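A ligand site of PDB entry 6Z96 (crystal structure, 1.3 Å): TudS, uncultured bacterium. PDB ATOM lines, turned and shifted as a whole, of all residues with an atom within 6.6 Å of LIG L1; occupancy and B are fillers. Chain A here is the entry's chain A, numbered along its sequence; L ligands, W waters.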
ATOM      1  N   VAL A   7     -25.615  21.275  -0.131  1.00  0.00           N
ATOM      2  CA  VAL A   7     -26.874  20.628  -0.482  1.00  0.00           C
ATOM      3  C   VAL A   7     -26.794  20.055  -1.881  1.00  0.00           C
ATOM      4  O   VAL A   7     -26.363  20.768  -2.776  1.00  0.00           O
ATOM      5  CB  VAL A   7     -28.055  21.649  -0.460  1.00  0.00           C
ATOM      6  CG1 VAL A   7     -29.391  20.968  -0.720  1.00  0.00           C
ATOM      7  CG2 VAL A   7     -28.083  22.422   0.856  1.00  0.00           C
ATOM      8  N   SER A   8     -27.258  18.818  -2.110  1.00  0.00           N
ATOM      9  CA  SER A   8     -27.340  18.251  -3.466  1.00  0.00           C
ATOM     10  C   SER A   8     -28.099  19.238  -4.373  1.00  0.00           C
ATOM     11  O   SER A   8     -29.196  19.654  -4.027  1.00  0.00           O
ATOM     12  CB  SER A   8     -28.150  16.960  -3.437  1.00  0.00           C
ATOM     13  OG  SER A   8     -27.396  15.910  -2.863  1.00  0.00           O
ATOM     14  N   ALA A   9     -27.477  19.641  -5.484  1.00  0.00           N
ATOM     15  CA  ALA A   9     -28.073  20.662  -6.345  1.00  0.00           C
ATOM     16  C   ALA A   9     -29.462  20.295  -6.848  1.00  0.00           C
ATOM     17  O   ALA A   9     -30.311  21.184  -7.008  1.00  0.00           O
ATOM     18  CB  ALA A   9     -27.147  20.981  -7.516  1.00  0.00           C
ATOM     19  N   CYS A  10     -29.721  18.993  -7.048  1.00  0.00           N
ATOM     20  CA  CYS A  10     -31.038  18.562  -7.510  1.00  0.00           C
ATOM     21  C   CYS A  10     -32.130  18.858  -6.458  1.00  0.00           C
ATOM     22  O   CYS A  10     -33.266  19.131  -6.842  1.00  0.00           O
ATOM     23  CB  CYS A  10     -31.041  17.099  -7.907  1.00  0.00           C
ATOM     24  SG  CYS A  10     -30.534  15.988  -6.571  1.00  0.00           S
ATOM     25  N   LEU A  11     -31.770  18.808  -5.162  1.00  0.00           N
ATOM     26  CA  LEU A  11     -32.782  19.096  -4.112  1.00  0.00           C
ATOM     27  C   LEU A  11     -33.201  20.561  -4.130  1.00  0.00           C
ATOM     28  O   LEU A  11     -34.266  20.893  -3.599  1.00  0.00           O
ATOM     29  CB  LEU A  11     -32.234  18.752  -2.726  1.00  0.00           C
ATOM     30  CG  LEU A  11     -31.989  17.249  -2.501  1.00  0.00           C
ATOM     31  CD1 LEU A  11     -31.327  17.019  -1.119  1.00  0.00           C
ATOM     32  CD2 LEU A  11     -33.298  16.455  -2.545  1.00  0.00           C
ATOM     33  N   GLN A  14     -32.328  22.261  -9.275  1.00  0.00           N
ATOM     34  CA  GLN A  14     -31.475  22.351 -10.456  1.00  0.00           C
ATOM     35  C   GLN A  14     -31.613  21.105 -11.308  1.00  0.00           C
ATOM     36  O   GLN A  14     -31.658  20.000 -10.791  1.00  0.00           O
ATOM     37  CB  GLN A  14     -30.049  22.611 -10.051  1.00  0.00           C
ATOM     38  CG  GLN A  14     -29.908  23.883  -9.212  1.00  0.00           C
ATOM     39  CD  GLN A  14     -28.492  24.317  -9.099  1.00  0.00           C
ATOM     40  OE1 GLN A  14     -27.639  23.958  -9.919  1.00  0.00           O
ATOM     41  NE2 GLN A  14     -28.200  25.165  -8.126  1.00  0.00           N
ATOM     42  N   VAL A  16     -29.924  18.931 -12.852  1.00  0.00           N
ATOM     43  CA  VAL A  16     -28.656  18.226 -12.997  1.00  0.00           C
ATOM     44  C   VAL A  16     -28.764  16.711 -12.815  1.00  0.00           C
ATOM     45  O   VAL A  16     -27.732  16.057 -12.878  1.00  0.00           O
ATOM     46  CB  VAL A  16     -27.624  18.811 -12.011  1.00  0.00           C
ATOM     47  CG1 VAL A  16     -27.217  20.234 -12.394  1.00  0.00           C
ATOM     48  CG2 VAL A  16     -28.150  18.745 -10.570  1.00  0.00           C
ATOM     49  N   ARG A  17     -29.979  16.139 -12.583  1.00  0.00           N
ATOM     50  CA  ARG A  17     -30.118  14.696 -12.397  1.00  0.00           C
ATOM     51  C   ARG A  17     -29.689  13.964 -13.661  1.00  0.00           C
ATOM     52  O   ARG A  17     -29.647  14.579 -14.751  1.00  0.00           O
ATOM     53  CB  ARG A  17     -31.574  14.336 -12.035  1.00  0.00           C
ATOM     54  CG  ARG A  17     -31.930  14.685 -10.581  1.00  0.00           C
ATOM     55  CD  ARG A  17     -31.430  13.635  -9.579  1.00  0.00           C
ATOM     56  NE  ARG A  17     -32.221  12.390  -9.670  1.00  0.00           N
ATOM     57  CZ  ARG A  17     -32.056  11.335  -8.891  1.00  0.00           C
ATOM     58  NH1 ARG A  17     -31.133  11.343  -7.923  1.00  0.00           N
ATOM     59  NH2 ARG A  17     -32.830  10.261  -9.042  1.00  0.00           N
ATOM     60  N   TYR A  18     -29.445  12.645 -13.545  1.00  0.00           N
ATOM     61  CA  TYR A  18     -29.005  11.859 -14.690  1.00  0.00           C
ATOM     62  C   TYR A  18     -30.009  11.938 -15.858  1.00  0.00           C
ATOM     63  O   TYR A  18     -29.601  11.816 -17.008  1.00  0.00           O
ATOM     64  CB  TYR A  18     -28.758  10.395 -14.285  1.00  0.00           C
ATOM     65  CG  TYR A  18     -30.018   9.594 -14.057  1.00  0.00           C
ATOM     66  CD1 TYR A  18     -30.767   9.777 -12.906  1.00  0.00           C
ATOM     67  CD2 TYR A  18     -30.506   8.740 -15.026  1.00  0.00           C
ATOM     68  CE1 TYR A  18     -31.964   9.091 -12.712  1.00  0.00           C
ATOM     69  CE2 TYR A  18     -31.705   8.061 -14.855  1.00  0.00           C
ATOM     70  CZ  TYR A  18     -32.418   8.209 -13.672  1.00  0.00           C
ATOM     71  OH  TYR A  18     -33.587   7.506 -13.469  1.00  0.00           O
ATOM     72  N   GLN A  21     -33.841  15.813 -15.011  1.00  0.00           N
ATOM     73  CA  GLN A  21     -34.907  16.313 -14.125  1.00  0.00           C
ATOM     74  C   GLN A  21     -34.301  16.975 -12.850  1.00  0.00           C
ATOM     75  O   GLN A  21     -33.095  17.043 -12.678  1.00  0.00           O
ATOM     76  CB  GLN A  21     -35.829  15.160 -13.694  1.00  0.00           C
ATOM     77  CG  GLN A  21     -36.670  14.572 -14.823  1.00  0.00           C
ATOM     78  CD  GLN A  21     -37.715  13.648 -14.251  1.00  0.00           C
ATOM     79  OE1 GLN A  21     -37.415  12.654 -13.564  1.00  0.00           O
ATOM     80  NE2 GLN A  21     -38.981  13.971 -14.512  1.00  0.00           N
ATOM     81  N   LYS A  23     -35.041  17.390  -8.344  1.00  0.00           N
ATOM     82  CA  LYS A  23     -35.678  16.768  -7.181  1.00  0.00           C
ATOM     83  C   LYS A  23     -35.947  17.865  -6.178  1.00  0.00           C
ATOM     84  O   LYS A  23     -35.645  17.738  -4.978  1.00  0.00           O
ATOM     85  CB  LYS A  23     -34.715  15.732  -6.571  1.00  0.00           C
ATOM     86  CG  LYS A  23     -34.487  14.525  -7.481  1.00  0.00           C
ATOM     87  CD  LYS A  23     -35.788  13.747  -7.659  1.00  0.00           C
ATOM     88  CE  LYS A  23     -35.607  12.397  -8.309  1.00  0.00           C
ATOM     89  NZ  LYS A  23     -36.926  11.726  -8.546  1.00  0.00           N
ATOM     90  N   PHE A  42     -24.428  21.859  -4.706  1.00  0.00           N
ATOM     91  CA  PHE A  42     -23.289  21.123  -5.249  1.00  0.00           C
ATOM     92  C   PHE A  42     -23.793  19.852  -5.850  1.00  0.00           C
ATOM     93  O   PHE A  42     -24.610  19.169  -5.244  1.00  0.00           O
ATOM     94  CB  PHE A  42     -22.266  20.807  -4.119  1.00  0.00           C
ATOM     95  CG  PHE A  42     -20.999  20.192  -4.656  1.00  0.00           C
ATOM     96  CD1 PHE A  42     -20.804  18.820  -4.613  1.00  0.00           C
ATOM     97  CD2 PHE A  42     -20.024  20.981  -5.235  1.00  0.00           C
ATOM     98  CE1 PHE A  42     -19.658  18.246  -5.165  1.00  0.00           C
ATOM     99  CE2 PHE A  42     -18.860  20.393  -5.767  1.00  0.00           C
ATOM    100  CZ  PHE A  42     -18.704  19.030  -5.713  1.00  0.00           C
ATOM    101  N   CYS A  43     -23.271  19.501  -7.041  1.00  0.00           N
ATOM    102  CA  CYS A  43     -23.623  18.208  -7.642  1.00  0.00           C
ATOM    103  C   CYS A  43     -22.319  17.461  -7.881  1.00  0.00           C
ATOM    104  O   CYS A  43     -21.575  17.811  -8.788  1.00  0.00           O
ATOM    105  CB  CYS A  43     -24.375  18.356  -8.972  1.00  0.00           C
ATOM    106  SG  CYS A  43     -24.609  16.784  -9.825  1.00  0.00           S
ATOM    107  N   PRO A  44     -22.047  16.398  -7.127  1.00  0.00           N
ATOM    108  CA  PRO A  44     -20.776  15.679  -7.315  1.00  0.00           C
ATOM    109  C   PRO A  44     -20.579  15.113  -8.724  1.00  0.00           C
ATOM    110  O   PRO A  44     -19.453  15.118  -9.201  1.00  0.00           O
ATOM    111  CB  PRO A  44     -20.873  14.530  -6.291  1.00  0.00           C
ATOM    112  CG  PRO A  44     -21.844  15.052  -5.213  1.00  0.00           C
ATOM    113  CD  PRO A  44     -22.823  15.914  -5.967  1.00  0.00           C
ATOM    114  N   GLU A  45     -21.660  14.624  -9.364  1.00  0.00           N
ATOM    115  CA  GLU A  45     -21.468  14.011 -10.680  1.00  0.00           C
ATOM    116  C   GLU A  45     -21.114  15.030 -11.740  1.00  0.00           C
ATOM    117  O   GLU A  45     -20.213  14.776 -12.558  1.00  0.00           O
ATOM    118  CB  GLU A  45     -22.641  13.142 -11.071  1.00  0.00           C
ATOM    119  CG  GLU A  45     -22.620  11.911 -10.183  1.00  0.00           C
ATOM    120  CD  GLU A  45     -23.905  11.099 -10.171  1.00  0.00           C
ATOM    121  OE1 GLU A  45     -24.621  11.121 -11.196  1.00  0.00           O
ATOM    122  OE2 GLU A  45     -24.180  10.397  -9.163  1.00  0.00           O
ATOM    123  N   VAL A  46     -21.772  16.186 -11.709  1.00  0.00           N
ATOM    124  CA  VAL A  46     -21.448  17.242 -12.669  1.00  0.00           C
ATOM    125  C   VAL A  46     -20.070  17.831 -12.330  1.00  0.00           C
ATOM    126  O   VAL A  46     -19.245  18.040 -13.230  1.00  0.00           O
ATOM    127  CB  VAL A  46     -22.550  18.313 -12.682  1.00  0.00           C
ATOM    128  CG1 VAL A  46     -22.116  19.535 -13.466  1.00  0.00           C
ATOM    129  CG2 VAL A  46     -23.845  17.740 -13.268  1.00  0.00           C
ATOM    130  N   ARG A  54     -27.029  11.634 -18.377  1.00  0.00           N
ATOM    131  CA  ARG A  54     -25.979  10.630 -18.299  1.00  0.00           C
ATOM    132  C   ARG A  54     -26.657   9.314 -17.947  1.00  0.00           C
ATOM    133  O   ARG A  54     -27.758   9.306 -17.387  1.00  0.00           O
ATOM    134  CB  ARG A  54     -24.905  11.048 -17.259  1.00  0.00           C
ATOM    135  CG  ARG A  54     -25.484  11.359 -15.907  1.00  0.00           C
ATOM    136  CD  ARG A  54     -24.394  11.949 -15.016  1.00  0.00           C
ATOM    137  NE  ARG A  54     -24.941  12.373 -13.718  1.00  0.00           N
ATOM    138  CZ  ARG A  54     -25.581  13.512 -13.500  1.00  0.00           C
ATOM    139  NH1 ARG A  54     -25.774  14.379 -14.501  1.00  0.00           N
ATOM    140  NH2 ARG A  54     -26.081  13.792 -12.304  1.00  0.00           N
ATOM    141  N   PHE A  76     -16.895   9.881 -10.204  1.00  0.00           N
ATOM    142  CA  PHE A  76     -17.593   9.861  -8.912  1.00  0.00           C
ATOM    143  C   PHE A  76     -16.618  10.223  -7.777  1.00  0.00           C
ATOM    144  O   PHE A  76     -16.982  10.978  -6.877  1.00  0.00           O
ATOM    145  CB  PHE A  76     -18.195   8.477  -8.632  1.00  0.00           C
ATOM    146  CG  PHE A  76     -19.573   8.343  -9.204  1.00  0.00           C
ATOM    147  CD1 PHE A  76     -19.770   8.322 -10.577  1.00  0.00           C
ATOM    148  CD2 PHE A  76     -20.682   8.275  -8.374  1.00  0.00           C
ATOM    149  CE1 PHE A  76     -21.049   8.224 -11.104  1.00  0.00           C
ATOM    150  CE2 PHE A  76     -21.960   8.169  -8.908  1.00  0.00           C
ATOM    151  CZ  PHE A  76     -22.137   8.144 -10.272  1.00  0.00           C
ATOM    152  N   LEU A  97     -28.049  15.699   1.427  1.00  0.00           N
ATOM    153  CA  LEU A  97     -27.820  15.034   0.147  1.00  0.00           C
ATOM    154  C   LEU A  97     -28.984  14.146  -0.251  1.00  0.00           C
ATOM    155  O   LEU A  97     -29.676  13.612   0.597  1.00  0.00           O
ATOM    156  CB  LEU A  97     -26.522  14.218   0.201  1.00  0.00           C
ATOM    157  CG  LEU A  97     -25.250  14.999   0.546  1.00  0.00           C
ATOM    158  CD1 LEU A  97     -23.993  14.061   0.440  1.00  0.00           C
ATOM    159  CD2 LEU A  97     -25.044  16.223  -0.354  1.00  0.00           C
ATOM    160  N   LYS A  98     -29.176  13.977  -1.569  1.00  0.00           N
ATOM    161  CA  LYS A  98     -30.287  13.201  -2.117  1.00  0.00           C
ATOM    162  C   LYS A  98     -30.207  11.694  -1.839  1.00  0.00           C
ATOM    163  O   LYS A  98     -29.268  11.020  -2.200  1.00  0.00           O
ATOM    164  CB  LYS A  98     -30.352  13.458  -3.651  1.00  0.00           C
ATOM    165  CG  LYS A  98     -31.406  12.621  -4.388  1.00  0.00           C
ATOM    166  CD  LYS A  98     -32.817  13.132  -4.072  1.00  0.00           C
ATOM    167  CE  LYS A  98     -33.849  12.129  -4.567  1.00  0.00           C
ATOM    168  NZ  LYS A  98     -34.018  10.986  -3.611  1.00  0.00           N
ATOM    169  N   GLU A  99     -31.293  11.152  -1.270  1.00  0.00           N
ATOM    170  CA  GLU A  99     -31.330   9.737  -0.925  1.00  0.00           C
ATOM    171  C   GLU A  99     -31.330   8.819  -2.168  1.00  0.00           C
ATOM    172  O   GLU A  99     -31.850   9.191  -3.222  1.00  0.00           O
ATOM    173  CB  GLU A  99     -32.574   9.450  -0.057  1.00  0.00           C
ATOM    174  CG  GLU A  99     -32.597   8.056   0.551  1.00  0.00           C
ATOM    175  CD  GLU A  99     -31.395   7.747   1.434  1.00  0.00           C
ATOM    176  OE1 GLU A  99     -30.293   7.522   0.885  1.00  0.00           O
ATOM    177  OE2 GLU A  99     -31.572   7.662   2.667  1.00  0.00           O
ATOM    178  N   SER A 101     -28.984   7.850  -4.188  1.00  0.00           N
ATOM    179  CA  SER A 101     -28.019   8.092  -5.267  1.00  0.00           C
ATOM    180  C   SER A 101     -26.670   7.364  -5.057  1.00  0.00           C
ATOM    181  O   SER A 101     -26.177   7.283  -3.934  1.00  0.00           O
ATOM    182  CB  SER A 101     -27.792   9.613  -5.368  1.00  0.00           C
ATOM    183  OG  SER A 101     -26.575   9.970  -6.021  1.00  0.00           O
ATOM    184  N   PRO A 102     -26.022   6.940  -6.153  1.00  0.00           N
ATOM    185  CA  PRO A 102     -24.674   6.346  -6.012  1.00  0.00           C
ATOM    186  C   PRO A 102     -23.625   7.369  -5.564  1.00  0.00           C
ATOM    187  O   PRO A 102     -22.552   6.948  -5.140  1.00  0.00           O
ATOM    188  CB  PRO A 102     -24.384   5.813  -7.419  1.00  0.00           C
ATOM    189  CG  PRO A 102     -25.209   6.675  -8.343  1.00  0.00           C
ATOM    190  CD  PRO A 102     -26.473   6.995  -7.564  1.00  0.00           C
ATOM    191  N   SER A 103     -23.922   8.686  -5.632  1.00  0.00           N
ATOM    192  CA  SER A 103     -23.080   9.736  -5.070  1.00  0.00           C
ATOM    193  C   SER A 103     -23.617  10.182  -3.718  1.00  0.00           C
ATOM    194  O   SER A 103     -22.869  10.231  -2.747  1.00  0.00           O
ATOM    195  CB  SER A 103     -23.036  10.983  -5.959  1.00  0.00           C
ATOM    196  OG  SER A 103     -22.300  10.775  -7.146  1.00  0.00           O
ATOM    197  N   CYS A 104     -24.893  10.568  -3.679  1.00  0.00           N
ATOM    198  CA  CYS A 104     -25.498  11.293  -2.568  1.00  0.00           C
ATOM    199  C   CYS A 104     -26.294  10.458  -1.586  1.00  0.00           C
ATOM    200  O   CYS A 104     -26.654  10.987  -0.518  1.00  0.00           O
ATOM    201  CB  CYS A 104     -26.358  12.419  -3.159  1.00  0.00           C
ATOM    202  SG  CYS A 104     -25.367  13.650  -4.072  1.00  0.00           S
ATOM    203  N   GLY A 105     -26.554   9.192  -1.883  1.00  0.00           N
ATOM    204  CA  GLY A 105     -27.340   8.348  -0.978  1.00  0.00           C
ATOM    205  C   GLY A 105     -26.740   8.262   0.412  1.00  0.00           C
ATOM    206  O   GLY A 105     -25.512   8.352   0.550  1.00  0.00           O
HETATM  207 FE1  LIG L   1     -27.337  13.116  -8.595  1.00  0.00          FE
HETATM  208 FE2  LIG L   1     -28.492  15.178  -7.263  1.00  0.00          FE
HETATM  209 FE3  LIG L   1     -26.054  15.543  -8.492  1.00  0.00          FE
HETATM  210 FE4  LIG L   1     -26.257  14.036  -6.208  1.00  0.00          FE
HETATM  211  S1  LIG L   1     -26.627  16.304  -6.448  1.00  0.00           S
HETATM  212  S2  LIG L   1     -25.050  13.502  -8.060  1.00  0.00           S
HETATM  213  S3  LIG L   1     -28.305  13.003  -6.528  1.00  0.00           S
HETATM  214  S4  LIG L   1     -28.092  15.114  -9.499  1.00  0.00           S
HETATM  215  S1  LG2 L   2     -28.163  11.825 -10.393  1.00  0.00           S
HETATM  216  O   HOH W   1     -26.791  10.429  -8.591  1.00  0.00           O
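S1 of LG2 L2 binds FE1 of LIG L1 (2.4 Å).
The backbone NH (N) of Tyr 18 sits close to a sulfur (S1) of LG2 L2 (3.5 Å). An iron atom (FE3) of LIG L1 is bound by the side-chain sulfur of Cys 43 (2.3 Å). FE4 of LIG L1 is bound by SG of Cys 104 (2.3 Å). FE2 of LIG L1 is bound by SG of Cys 10 (2.3 Å). The side-chain hydroxyl (OG) of Ser 101 lies close to a sulfur (S3) of LIG L1 (3.5 Å). The guanidinium group (NH2) of Arg 54 sits close to a sulfur (S4) of LIG L1 (3.7 Å). The guanidinium group of Arg 17 lies close to a sulfur (S3) of LIG L1 (3.6 Å). OE1 of Glu 45 lies close to S1 of LG2 L2 (3.7 Å). The side-chain hydroxyl (OG) of Ser 8 lies close to a sulfur (S1) of LIG L1 (3.7 Å). The backbone NH (N) of Arg 17 lies close to a sulfur (S4) of LIG L1. N of Ala 9 sits close to S1 of LIG L1 (3.6 Å). The guanidinium group (NH2) of Arg 54 lies close to a sulfur (S1) of LG2 L2.
The backbone NH (N) of Ala 9 lies within hydrogen-bond range of the backbone carbonyl oxygen (O) of Phe 42 (2.9 Å). The guanidinium group of Arg 54 sits at hydrogen-bond distance from the backbone carbonyl oxygen of Val 16 (2.9 Å). The backbone NH (N) of Arg 54 lies within hydrogen-bond range of the backbone carbonyl oxygen (O) of Tyr 18, 2.9 Å away. OG of Ser 101 lies within hydrogen-bond range of N of Ser 103 (3.0 Å). The backbone NH (N) of Glu 45 sits close to the side-chain sulfur (SG) of Cys 43, 3.7 Å away. O of Ala 9 lies within hydrogen-bond range of N of Gln 14 (3.2 Å). The backbone NH of Cys 104 sits at hydrogen-bond distance from the side-chain hydroxyl of Ser 101 (2.9 Å). OG of Ser 103 lies within hydrogen-bond range of OE2 of Glu 45 (2.8 Å).
The backbone carbonyl oxygen (O) of Val 16 lies close to a sulfur (S4) of LIG L1, at 3.5 Å. O of Phe 42 sits close to S1 of LIG L1. The side-chain carboxylate (OE2) of Glu 45 sits close to a sulfur (S2) of LIG L1 (3.4 Å). Merely in contact with LIG L1: Lys 98 (3.6 Å), Ser 103 (3.8 Å) and Pro 44 (3.9 Å). Within 4 Å of LIG L1: Ser 8, Ala 9, Cys 10, Val 16, Arg 17, Phe 42, Cys 43, Pro 44, Glu 45, Arg 54, Lys 98, Ser 101, Ser 103 and Cys 104. The nearest printed residue that does not touch LIG L1 is Tyr 18 (4.9 Å).
Water W1 lies within hydrogen-bond range of the side-chain hydroxyl (OG) of Ser 101 (2.6 Å), the side-chain carboxylate (OE2) of Glu 45 (2.7 Å) and a sulfur (S2) of LIG L1 (3.6 Å).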
